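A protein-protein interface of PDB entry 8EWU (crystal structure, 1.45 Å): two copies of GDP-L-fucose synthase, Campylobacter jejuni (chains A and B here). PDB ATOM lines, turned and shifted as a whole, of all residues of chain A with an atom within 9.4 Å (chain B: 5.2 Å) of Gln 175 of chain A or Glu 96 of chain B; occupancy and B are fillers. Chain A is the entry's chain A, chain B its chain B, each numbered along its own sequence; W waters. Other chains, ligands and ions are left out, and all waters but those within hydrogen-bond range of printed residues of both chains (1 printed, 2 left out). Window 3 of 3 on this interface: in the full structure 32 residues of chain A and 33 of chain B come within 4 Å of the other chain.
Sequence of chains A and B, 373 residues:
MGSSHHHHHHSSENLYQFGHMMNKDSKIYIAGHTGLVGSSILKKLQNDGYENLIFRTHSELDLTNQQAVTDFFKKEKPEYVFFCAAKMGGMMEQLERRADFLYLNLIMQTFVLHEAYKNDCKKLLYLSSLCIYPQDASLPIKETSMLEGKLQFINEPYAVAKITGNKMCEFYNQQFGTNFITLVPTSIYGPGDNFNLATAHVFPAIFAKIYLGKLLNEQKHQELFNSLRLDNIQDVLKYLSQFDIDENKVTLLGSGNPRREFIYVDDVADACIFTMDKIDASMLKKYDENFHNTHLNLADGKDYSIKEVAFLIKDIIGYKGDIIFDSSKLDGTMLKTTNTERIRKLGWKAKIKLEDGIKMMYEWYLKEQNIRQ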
ATOM      1  N   HIS A 114      -3.990  18.983  24.126  1.00  0.00           N
ATOM      2  CA  HIS A 114      -3.889  19.336  22.693  1.00  0.00           C
ATOM      3  C   HIS A 114      -2.563  20.040  22.411  1.00  0.00           C
ATOM      4  O   HIS A 114      -1.864  19.647  21.431  1.00  0.00           O
ATOM      5  CB  HIS A 114      -5.078  20.154  22.214  1.00  0.00           C
ATOM      6  CG  HIS A 114      -5.046  20.382  20.753  1.00  0.00           C
ATOM      7  ND1 HIS A 114      -5.270  19.399  19.834  1.00  0.00           N
ATOM      8  CD2 HIS A 114      -4.812  21.512  20.070  1.00  0.00           C
ATOM      9  CE1 HIS A 114      -5.143  19.910  18.615  1.00  0.00           C
ATOM     10  NE2 HIS A 114      -4.851  21.194  18.739  1.00  0.00           N
ATOM     11  N   TYR A 117       0.461  17.781  22.400  1.00  0.00           N
ATOM     12  CA  TYR A 117       0.539  17.097  21.091  1.00  0.00           C
ATOM     13  C   TYR A 117       1.091  18.041  20.006  1.00  0.00           C
ATOM     14  O   TYR A 117       2.018  17.630  19.265  1.00  0.00           O
ATOM     15  CB  TYR A 117      -0.828  16.526  20.699  1.00  0.00           C
ATOM     16  CG  TYR A 117      -0.992  16.403  19.216  1.00  0.00           C
ATOM     17  CD1 TYR A 117      -0.293  15.459  18.484  1.00  0.00           C
ATOM     18  CD2 TYR A 117      -1.802  17.295  18.520  1.00  0.00           C
ATOM     19  CE1 TYR A 117      -0.406  15.380  17.108  1.00  0.00           C
ATOM     20  CE2 TYR A 117      -1.914  17.233  17.146  1.00  0.00           C
ATOM     21  CZ  TYR A 117      -1.207  16.287  16.438  1.00  0.00           C
ATOM     22  OH  TYR A 117      -1.355  16.235  15.080  1.00  0.00           O
ATOM     23  N   LYS A 167     -10.588   9.322  27.523  1.00  0.00           N
ATOM     24  CA  LYS A 167     -10.863   8.961  26.118  1.00  0.00           C
ATOM     25  C   LYS A 167     -10.032   9.845  25.177  1.00  0.00           C
ATOM     26  O   LYS A 167      -9.486   9.324  24.189  1.00  0.00           O
ATOM     27  CB  LYS A 167     -12.359   9.021  25.807  1.00  0.00           C
ATOM     28  CG  LYS A 167     -13.221   8.003  26.537  1.00  0.00           C
ATOM     29  CD  LYS A 167     -12.801   6.559  26.391  1.00  0.00           C
ATOM     30  CE  LYS A 167     -13.165   5.950  25.068  1.00  0.00           C
ATOM     31  NZ  LYS A 167     -12.844   4.481  25.024  1.00  0.00           N
ATOM     32  N   MET A 168      -9.837  11.113  25.515  1.00  0.00           N
ATOM     33  CA  MET A 168      -8.980  11.992  24.689  1.00  0.00           C
ATOM     34  C   MET A 168      -7.561  11.433  24.593  1.00  0.00           C
ATOM     35  O   MET A 168      -6.989  11.402  23.482  1.00  0.00           O
ATOM     36  CB  MET A 168      -8.909  13.420  25.212  1.00  0.00           C
ATOM     37  CG  MET A 168      -8.127  14.345  24.299  1.00  0.00           C
ATOM     38  SD  MET A 168      -8.259  16.042  24.969  1.00  0.00           S
ATOM     39  CE  MET A 168      -7.228  17.024  23.862  1.00  0.00           C
ATOM     40  N   CYS A 169      -7.006  10.928  25.670  1.00  0.00           N
ATOM     41  CA  CYS A 169      -5.669  10.325  25.641  1.00  0.00           C
ATOM     42  C   CYS A 169      -5.720   9.147  24.686  1.00  0.00           C
ATOM     43  O   CYS A 169      -4.772   9.039  23.893  1.00  0.00           O
ATOM     44  CB  CYS A 169      -5.195   9.897  27.021  1.00  0.00           C
ATOM     45  SG  CYS A 169      -4.890  11.298  28.117  1.00  0.00           S
ATOM     46  N   GLU A 170      -6.707   8.242  24.812  1.00  0.00           N
ATOM     47  CA  GLU A 170      -6.810   7.052  23.923  1.00  0.00           C
ATOM     48  C   GLU A 170      -6.789   7.517  22.450  1.00  0.00           C
ATOM     49  O   GLU A 170      -6.143   6.902  21.553  1.00  0.00           O
ATOM     50  CB  GLU A 170      -8.073   6.244  24.146  1.00  0.00           C
ATOM     51  CG  GLU A 170      -8.194   5.665  25.519  1.00  0.00           C
ATOM     52  CD  GLU A 170      -9.431   4.815  25.715  1.00  0.00           C
ATOM     53  OE1 GLU A 170     -10.141   4.489  24.706  1.00  0.00           O
ATOM     54  OE2 GLU A 170      -9.676   4.481  26.893  1.00  0.00           O
ATOM     55  N   PHE A 171      -7.568   8.541  22.125  1.00  0.00           N
ATOM     56  CA  PHE A 171      -7.821   8.933  20.717  1.00  0.00           C
ATOM     57  C   PHE A 171      -6.572   9.592  20.151  1.00  0.00           C
ATOM     58  O   PHE A 171      -6.264   9.356  18.984  1.00  0.00           O
ATOM     59  CB  PHE A 171      -9.002   9.895  20.659  1.00  0.00           C
ATOM     60  CG  PHE A 171     -10.317   9.333  21.151  1.00  0.00           C
ATOM     61  CD1 PHE A 171     -10.625   7.978  21.144  1.00  0.00           C
ATOM     62  CD2 PHE A 171     -11.270  10.217  21.637  1.00  0.00           C
ATOM     63  CE1 PHE A 171     -11.842   7.523  21.623  1.00  0.00           C
ATOM     64  CE2 PHE A 171     -12.486   9.746  22.091  1.00  0.00           C
ATOM     65  CZ  PHE A 171     -12.767   8.407  22.128  1.00  0.00           C
ATOM     66  N   TYR A 172      -5.899  10.443  20.915  1.00  0.00           N
ATOM     67  CA  TYR A 172      -4.607  11.027  20.494  1.00  0.00           C
ATOM     68  C   TYR A 172      -3.587   9.897  20.312  1.00  0.00           C
ATOM     69  O   TYR A 172      -2.827   9.874  19.285  1.00  0.00           O
ATOM     70  CB  TYR A 172      -4.163  12.105  21.465  1.00  0.00           C
ATOM     71  CG  TYR A 172      -4.809  13.440  21.170  1.00  0.00           C
ATOM     72  CD1 TYR A 172      -6.168  13.629  21.293  1.00  0.00           C
ATOM     73  CD2 TYR A 172      -4.057  14.502  20.714  1.00  0.00           C
ATOM     74  CE1 TYR A 172      -6.770  14.851  21.036  1.00  0.00           C
ATOM     75  CE2 TYR A 172      -4.636  15.734  20.450  1.00  0.00           C
ATOM     76  CZ  TYR A 172      -5.992  15.921  20.614  1.00  0.00           C
ATOM     77  OH  TYR A 172      -6.580  17.124  20.279  1.00  0.00           O
ATOM     78  N   ASN A 173      -3.594   8.938  21.218  1.00  0.00           N
ATOM     79  CA  ASN A 173      -2.631   7.819  21.098  1.00  0.00           C
ATOM     80  C   ASN A 173      -2.908   7.080  19.791  1.00  0.00           C
ATOM     81  O   ASN A 173      -1.929   6.673  19.117  1.00  0.00           O
ATOM     82  CB  ASN A 173      -2.683   6.905  22.310  1.00  0.00           C
ATOM     83  CG  ASN A 173      -2.127   7.527  23.562  1.00  0.00           C
ATOM     84  OD1 ASN A 173      -1.459   8.567  23.542  1.00  0.00           O
ATOM     85  ND2 ASN A 173      -2.350   6.877  24.690  1.00  0.00           N
ATOM     86  N   GLN A 174      -4.181   6.838  19.484  1.00  0.00           N
ATOM     87  CA  GLN A 174      -4.572   6.055  18.285  1.00  0.00           C
ATOM     88  C   GLN A 174      -4.309   6.879  17.023  1.00  0.00           C
ATOM     89  O   GLN A 174      -3.654   6.313  16.059  1.00  0.00           O
ATOM     90  CB  GLN A 174      -6.014   5.566  18.309  1.00  0.00           C
ATOM     91  CG  GLN A 174      -6.353   4.692  17.101  1.00  0.00           C
ATOM     92  CD  GLN A 174      -5.856   3.274  17.250  1.00  0.00           C
ATOM     93  OE1 GLN A 174      -4.892   3.001  17.948  1.00  0.00           O
ATOM     94  NE2 GLN A 174      -6.552   2.331  16.660  1.00  0.00           N
ATOM     95  N   GLN A 175      -4.756   8.126  16.944  1.00  0.00           N
ATOM     96  CA  GLN A 175      -4.659   8.856  15.660  1.00  0.00           C
ATOM     97  C   GLN A 175      -3.236   9.366  15.426  1.00  0.00           C
ATOM     98  O   GLN A 175      -2.849   9.440  14.251  1.00  0.00           O
ATOM     99  CB  GLN A 175      -5.618  10.043  15.576  1.00  0.00           C
ATOM    100  CG  GLN A 175      -5.783  10.589  14.149  1.00  0.00           C
ATOM    101  CD  GLN A 175      -6.736  11.763  14.037  1.00  0.00           C
ATOM    102  OE1 GLN A 175      -7.566  11.982  14.927  1.00  0.00           O
ATOM    103  NE2 GLN A 175      -6.634  12.518  12.936  1.00  0.00           N
ATOM    104  N   PHE A 176      -2.537   9.791  16.483  1.00  0.00           N
ATOM    105  CA  PHE A 176      -1.312  10.612  16.346  1.00  0.00           C
ATOM    106  C   PHE A 176      -0.062   9.876  16.843  1.00  0.00           C
ATOM    107  O   PHE A 176       1.035  10.422  16.665  1.00  0.00           O
ATOM    108  CB  PHE A 176      -1.499  11.948  17.045  1.00  0.00           C
ATOM    109  CG  PHE A 176      -2.616  12.804  16.516  1.00  0.00           C
ATOM    110  CD1 PHE A 176      -2.863  12.897  15.156  1.00  0.00           C
ATOM    111  CD2 PHE A 176      -3.371  13.573  17.392  1.00  0.00           C
ATOM    112  CE1 PHE A 176      -3.881  13.712  14.680  1.00  0.00           C
ATOM    113  CE2 PHE A 176      -4.377  14.398  16.910  1.00  0.00           C
ATOM    114  CZ  PHE A 176      -4.645  14.441  15.558  1.00  0.00           C
ATOM    115  N   GLY A 177      -0.212   8.743  17.515  1.00  0.00           N
ATOM    116  CA  GLY A 177       0.942   7.998  18.043  1.00  0.00           C
ATOM    117  C   GLY A 177       1.577   8.711  19.222  1.00  0.00           C
ATOM    118  O   GLY A 177       2.800   8.530  19.446  1.00  0.00           O
ATOM    119  N   THR A 178       0.790   9.428  20.037  1.00  0.00           N
ATOM    120  CA  THR A 178       1.262  10.098  21.272  1.00  0.00           C
ATOM    121  C   THR A 178       1.493   9.030  22.356  1.00  0.00           C
ATOM    122  O   THR A 178       1.041   7.853  22.207  1.00  0.00           O
ATOM    123  CB  THR A 178       0.277  11.196  21.695  1.00  0.00           C
ATOM    124  OG1 THR A 178      -1.015  10.596  21.688  1.00  0.00           O
ATOM    125  CG2 THR A 178       0.249  12.375  20.761  1.00  0.00           C
ATOM    126  N   ASN A 290      -6.333  -1.338  20.589  1.00  0.00           N
ATOM    127  CA  ASN A 290      -6.965  -0.060  20.163  1.00  0.00           C
ATOM    128  C   ASN A 290      -6.974   0.983  21.301  1.00  0.00           C
ATOM    129  O   ASN A 290      -7.677   2.007  21.184  1.00  0.00           O
ATOM    130  CB  ASN A 290      -8.388  -0.308  19.681  1.00  0.00           C
ATOM    131  CG  ASN A 290      -8.377  -1.023  18.353  1.00  0.00           C
ATOM    132  OD1 ASN A 290      -7.774  -0.519  17.410  1.00  0.00           O
ATOM    133  ND2 ASN A 290      -9.017  -2.178  18.301  1.00  0.00           N
ATOM    134  N   PHE A 291      -6.168   0.762  22.343  1.00  0.00           N
ATOM    135  CA  PHE A 291      -6.010   1.694  23.486  1.00  0.00           C
ATOM    136  C   PHE A 291      -7.297   1.808  24.296  1.00  0.00           C
ATOM    137  O   PHE A 291      -7.350   2.621  25.232  1.00  0.00           O
ATOM    138  CB  PHE A 291      -5.609   3.104  23.048  1.00  0.00           C
ATOM    139  CG  PHE A 291      -4.251   3.157  22.402  1.00  0.00           C
ATOM    140  CD1 PHE A 291      -3.109   3.064  23.177  1.00  0.00           C
ATOM    141  CD2 PHE A 291      -4.134   3.215  21.026  1.00  0.00           C
ATOM    142  CE1 PHE A 291      -1.854   3.071  22.588  1.00  0.00           C
ATOM    143  CE2 PHE A 291      -2.878   3.228  20.435  1.00  0.00           C
ATOM    144  CZ  PHE A 291      -1.748   3.128  21.220  1.00  0.00           C
ATOM    145  N   MET B  92     -16.161   5.410   8.158  1.00  0.00           N
ATOM    146  CA  MET B  92     -14.720   5.194   7.872  1.00  0.00           C
ATOM    147  C   MET B  92     -13.911   6.429   8.267  1.00  0.00           C
ATOM    148  O   MET B  92     -12.847   6.236   8.866  1.00  0.00           O
ATOM    149  CB  MET B  92     -14.458   4.784   6.421  1.00  0.00           C
ATOM    150  CG  MET B  92     -15.172   3.516   6.063  1.00  0.00           C
ATOM    151  SD  MET B  92     -14.812   2.137   7.190  1.00  0.00           S
ATOM    152  CE  MET B  92     -13.065   1.938   6.842  1.00  0.00           C
ATOM    153  N   GLU B  93     -14.422   7.651   8.082  1.00  0.00           N
ATOM    154  CA  GLU B  93     -13.717   8.853   8.578  1.00  0.00           C
ATOM    155  C   GLU B  93     -13.636   8.775  10.110  1.00  0.00           C
ATOM    156  O   GLU B  93     -12.613   9.194  10.673  1.00  0.00           O
ATOM    157  CB  GLU B  93     -14.422  10.124   8.111  1.00  0.00           C
ATOM    158  CG  GLU B  93     -13.653  11.403   8.397  1.00  0.00           C
ATOM    159  CD  GLU B  93     -12.694  11.904   7.325  1.00  0.00           C
ATOM    160  OE1 GLU B  93     -12.578  13.134   7.192  1.00  0.00           O
ATOM    161  OE2 GLU B  93     -12.103  11.060   6.630  1.00  0.00           O
ATOM    162  N   GLN B  94     -14.703   8.301  10.755  1.00  0.00           N
ATOM    163  CA  GLN B  94     -14.718   8.231  12.245  1.00  0.00           C
ATOM    164  C   GLN B  94     -13.644   7.250  12.725  1.00  0.00           C
ATOM    165  O   GLN B  94     -13.017   7.501  13.784  1.00  0.00           O
ATOM    166  CB  GLN B  94     -16.082   7.775  12.750  1.00  0.00           C
ATOM    167  CG  GLN B  94     -17.132   8.860  12.643  1.00  0.00           C
ATOM    168  CD  GLN B  94     -18.457   8.377  13.182  1.00  0.00           C
ATOM    169  OE1 GLN B  94     -18.620   8.168  14.395  1.00  0.00           O
ATOM    170  NE2 GLN B  94     -19.400   8.206  12.263  1.00  0.00           N
ATOM    171  N   LEU B  95     -13.431   6.165  12.001  1.00  0.00           N
ATOM    172  CA  LEU B  95     -12.383   5.174  12.392  1.00  0.00           C
ATOM    173  C   LEU B  95     -10.988   5.775  12.250  1.00  0.00           C
ATOM    174  O   LEU B  95     -10.112   5.303  13.010  1.00  0.00           O
ATOM    175  CB  LEU B  95     -12.566   3.910  11.555  1.00  0.00           C
ATOM    176  CG  LEU B  95     -13.675   3.014  12.060  1.00  0.00           C
ATOM    177  CD1 LEU B  95     -13.946   1.913  11.072  1.00  0.00           C
ATOM    178  CD2 LEU B  95     -13.347   2.431  13.426  1.00  0.00           C
ATOM    179  N   GLU B  96     -10.770   6.768  11.398  1.00  0.00           N
ATOM    180  CA  GLU B  96      -9.452   7.425  11.262  1.00  0.00           C
ATOM    181  C   GLU B  96      -9.309   8.591  12.258  1.00  0.00           C
ATOM    182  O   GLU B  96      -8.298   8.639  13.008  1.00  0.00           O
ATOM    183  CB  GLU B  96      -9.253   7.864   9.821  1.00  0.00           C
ATOM    184  CG  GLU B  96      -7.936   8.585   9.597  1.00  0.00           C
ATOM    185  CD  GLU B  96      -6.680   7.826  10.018  1.00  0.00           C
ATOM    186  OE1 GLU B  96      -5.688   8.497  10.428  1.00  0.00           O
ATOM    187  OE2 GLU B  96      -6.673   6.576   9.919  1.00  0.00           O
ATOM    188  N   ARG B  97     -10.279   9.501  12.317  1.00  0.00           N
ATOM    189  CA  ARG B  97     -10.083  10.813  12.960  1.00  0.00           C
ATOM    190  C   ARG B  97     -10.575  10.727  14.410  1.00  0.00           C
ATOM    191  O   ARG B  97     -11.424  11.526  14.817  1.00  0.00           O
ATOM    192  CB  ARG B  97     -10.732  11.922  12.134  1.00  0.00           C
ATOM    193  CG  ARG B  97     -10.190  12.000  10.714  1.00  0.00           C
ATOM    194  CD  ARG B  97     -10.721  13.213   9.979  1.00  0.00           C
ATOM    195  NE  ARG B  97     -10.307  14.499  10.524  1.00  0.00           N
ATOM    196  CZ  ARG B  97     -10.652  15.691  10.018  1.00  0.00           C
ATOM    197  NH1 ARG B  97     -11.468  15.767   8.982  1.00  0.00           N
ATOM    198  NH2 ARG B  97     -10.220  16.809  10.560  1.00  0.00           N
ATOM    199  N   ARG B  98      -9.953   9.855  15.191  1.00  0.00           N
ATOM    200  CA  ARG B  98     -10.389   9.614  16.588  1.00  0.00           C
ATOM    201  C   ARG B  98     -10.190  10.892  17.379  1.00  0.00           C
ATOM    202  O   ARG B  98     -11.083  11.275  18.162  1.00  0.00           O
ATOM    203  CB  ARG B  98      -9.610   8.473  17.262  1.00  0.00           C
ATOM    204  CG  ARG B  98      -9.521   7.180  16.471  1.00  0.00           C
ATOM    205  CD  ARG B  98     -10.862   6.584  16.197  1.00  0.00           C
ATOM    206  NE  ARG B  98     -11.449   5.902  17.309  1.00  0.00           N
ATOM    207  CZ  ARG B  98     -12.633   5.353  17.246  1.00  0.00           C
ATOM    208  NH1 ARG B  98     -13.432   5.573  16.184  1.00  0.00           N
ATOM    209  NH2 ARG B  98     -13.067   4.733  18.316  1.00  0.00           N
ATOM    210  N   ALA B  99      -9.036  11.528  17.257  1.00  0.00           N
ATOM    211  CA  ALA B  99      -8.684  12.707  18.092  1.00  0.00           C
ATOM    212  C   ALA B  99      -9.490  13.897  17.595  1.00  0.00           C
ATOM    213  O   ALA B  99     -10.096  14.606  18.402  1.00  0.00           O
ATOM    214  CB  ALA B  99      -7.206  13.021  18.038  1.00  0.00           C
ATOM    215  N   ASP B 100      -9.543  14.070  16.274  1.00  0.00           N
ATOM    216  CA  ASP B 100     -10.132  15.300  15.672  1.00  0.00           C
ATOM    217  C   ASP B 100     -11.617  15.346  15.996  1.00  0.00           C
ATOM    218  O   ASP B 100     -12.112  16.402  16.337  1.00  0.00           O
ATOM    219  CB  ASP B 100     -10.004  15.322  14.162  1.00  0.00           C
ATOM    220  CG  ASP B 100      -8.569  15.328  13.650  1.00  0.00           C
ATOM    221  OD1 ASP B 100      -7.662  15.770  14.382  1.00  0.00           O
ATOM    222  OD2 ASP B 100      -8.414  14.798  12.538  1.00  0.00           O
HETATM  223  O   HOH W   1      -4.879  11.477  10.839  1.00  0.00           O
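No position is printed for both chains.
Of the 10 pairs that touch across the chains among the printed residues, none has its exchanged pair printed and touching as well.
Printed residues of chain A that touch a printed residue of chain B: Phe 171, Tyr 172, Gln 175 and Phe 176.
Among the printed residues, 10 pairs touch across the chains.
The side-chain amide oxygen (OE1) of Gln 175 of chain A is in hydrogen-bond range of the backbone NH (N) of Arg 98 of chain B.
The side-chain amide oxygen (OE1) of Gln 175 of chain A sits at hydrogen-bond distance from the backbone NH (N) of Ala 99 of chain B, at 2.8 Å.
The side-chain amide nitrogen (NE2) of Gln 175 of chain A is in hydrogen-bond range of the side-chain carboxylate (OD2) of Asp 100 of chain B.
Gln 175 of chain A touches just these residues of chain B: Glu 96 (3.4 Å), Arg 97 (3.3 Å), Arg 98 (3.2 Å), Ala 99 (2.8 Å) and Asp 100 (2.9 Å).
Glu 96 of chain B touches just one residue of chain A: Gln 175.
Printed residues of chain A within 4 Å of Arg 98 of chain B: Phe 171 (3.5 Å) and Gln 175 (3.2 Å).
Printed residues of chain A within 4 Å of Arg 97 of chain B: Gln 175.
Of the printed residues of chain A, Asp 100 of chain B touches Gln 175 and Phe 176.
Printed residues of chain B within 4 Å of Tyr 172 of chain A: Ala 99.
Printed residues of chain B within 4 Å of Phe 176 of chain A: Ala 99 and Asp 100.
The nearest printed residue of chain A that does not touch Glu 96 of chain B is Gln 174 of chain A (5.9 Å).
The nearest printed residue of chain B that does not touch Phe 176 of chain A is Arg 98 of chain B (6.8 Å).
ND1 of His 114 of chain A sits at hydrogen-bond distance from OH of Tyr 172 of chain A, at 2.7 Å.
O of Tyr 172 of chain A lies within hydrogen-bond range of N of Gly 177 of chain A, at 3.4 Å.
The side-chain hydroxyl (OG1) of Thr 178 of chain A lies close to the backbone carbonyl oxygen (O) of Tyr 172 of chain A (3.1 Å).
NH1 of Arg 97 of chain B is in salt-bridge range of OE1 of Glu 93 of chain B (3.4 Å).
NH1 of Arg 98 of chain B is in hydrogen-bond range of O of Gln 94 of chain B (3.1 Å).
OD2 of Asp 100 of chain B lies within salt-bridge range of NE of Arg 97 of chain B (2.8 Å).
Among the printed residues, pairs that only touch across the chains: Phe 171 of chain A with Arg 98 of chain B, Phe 171 of chain A with Ala 99 of chain B, Tyr 172 of chain A with Ala 99 of chain B, Gln 175 of chain A with Glu 96 of chain B, Gln 175 of chain A with Arg 97 of chain B, Phe 176 of chain A with Ala 99 of chain B and Phe 176 of chain A with Asp 100 of chain B.
Water W1 lies within hydrogen-bond range of NE2 of Gln 175 of chain A (2.9 Å) and OE1 of Glu 96 of chain B (3.1 Å).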
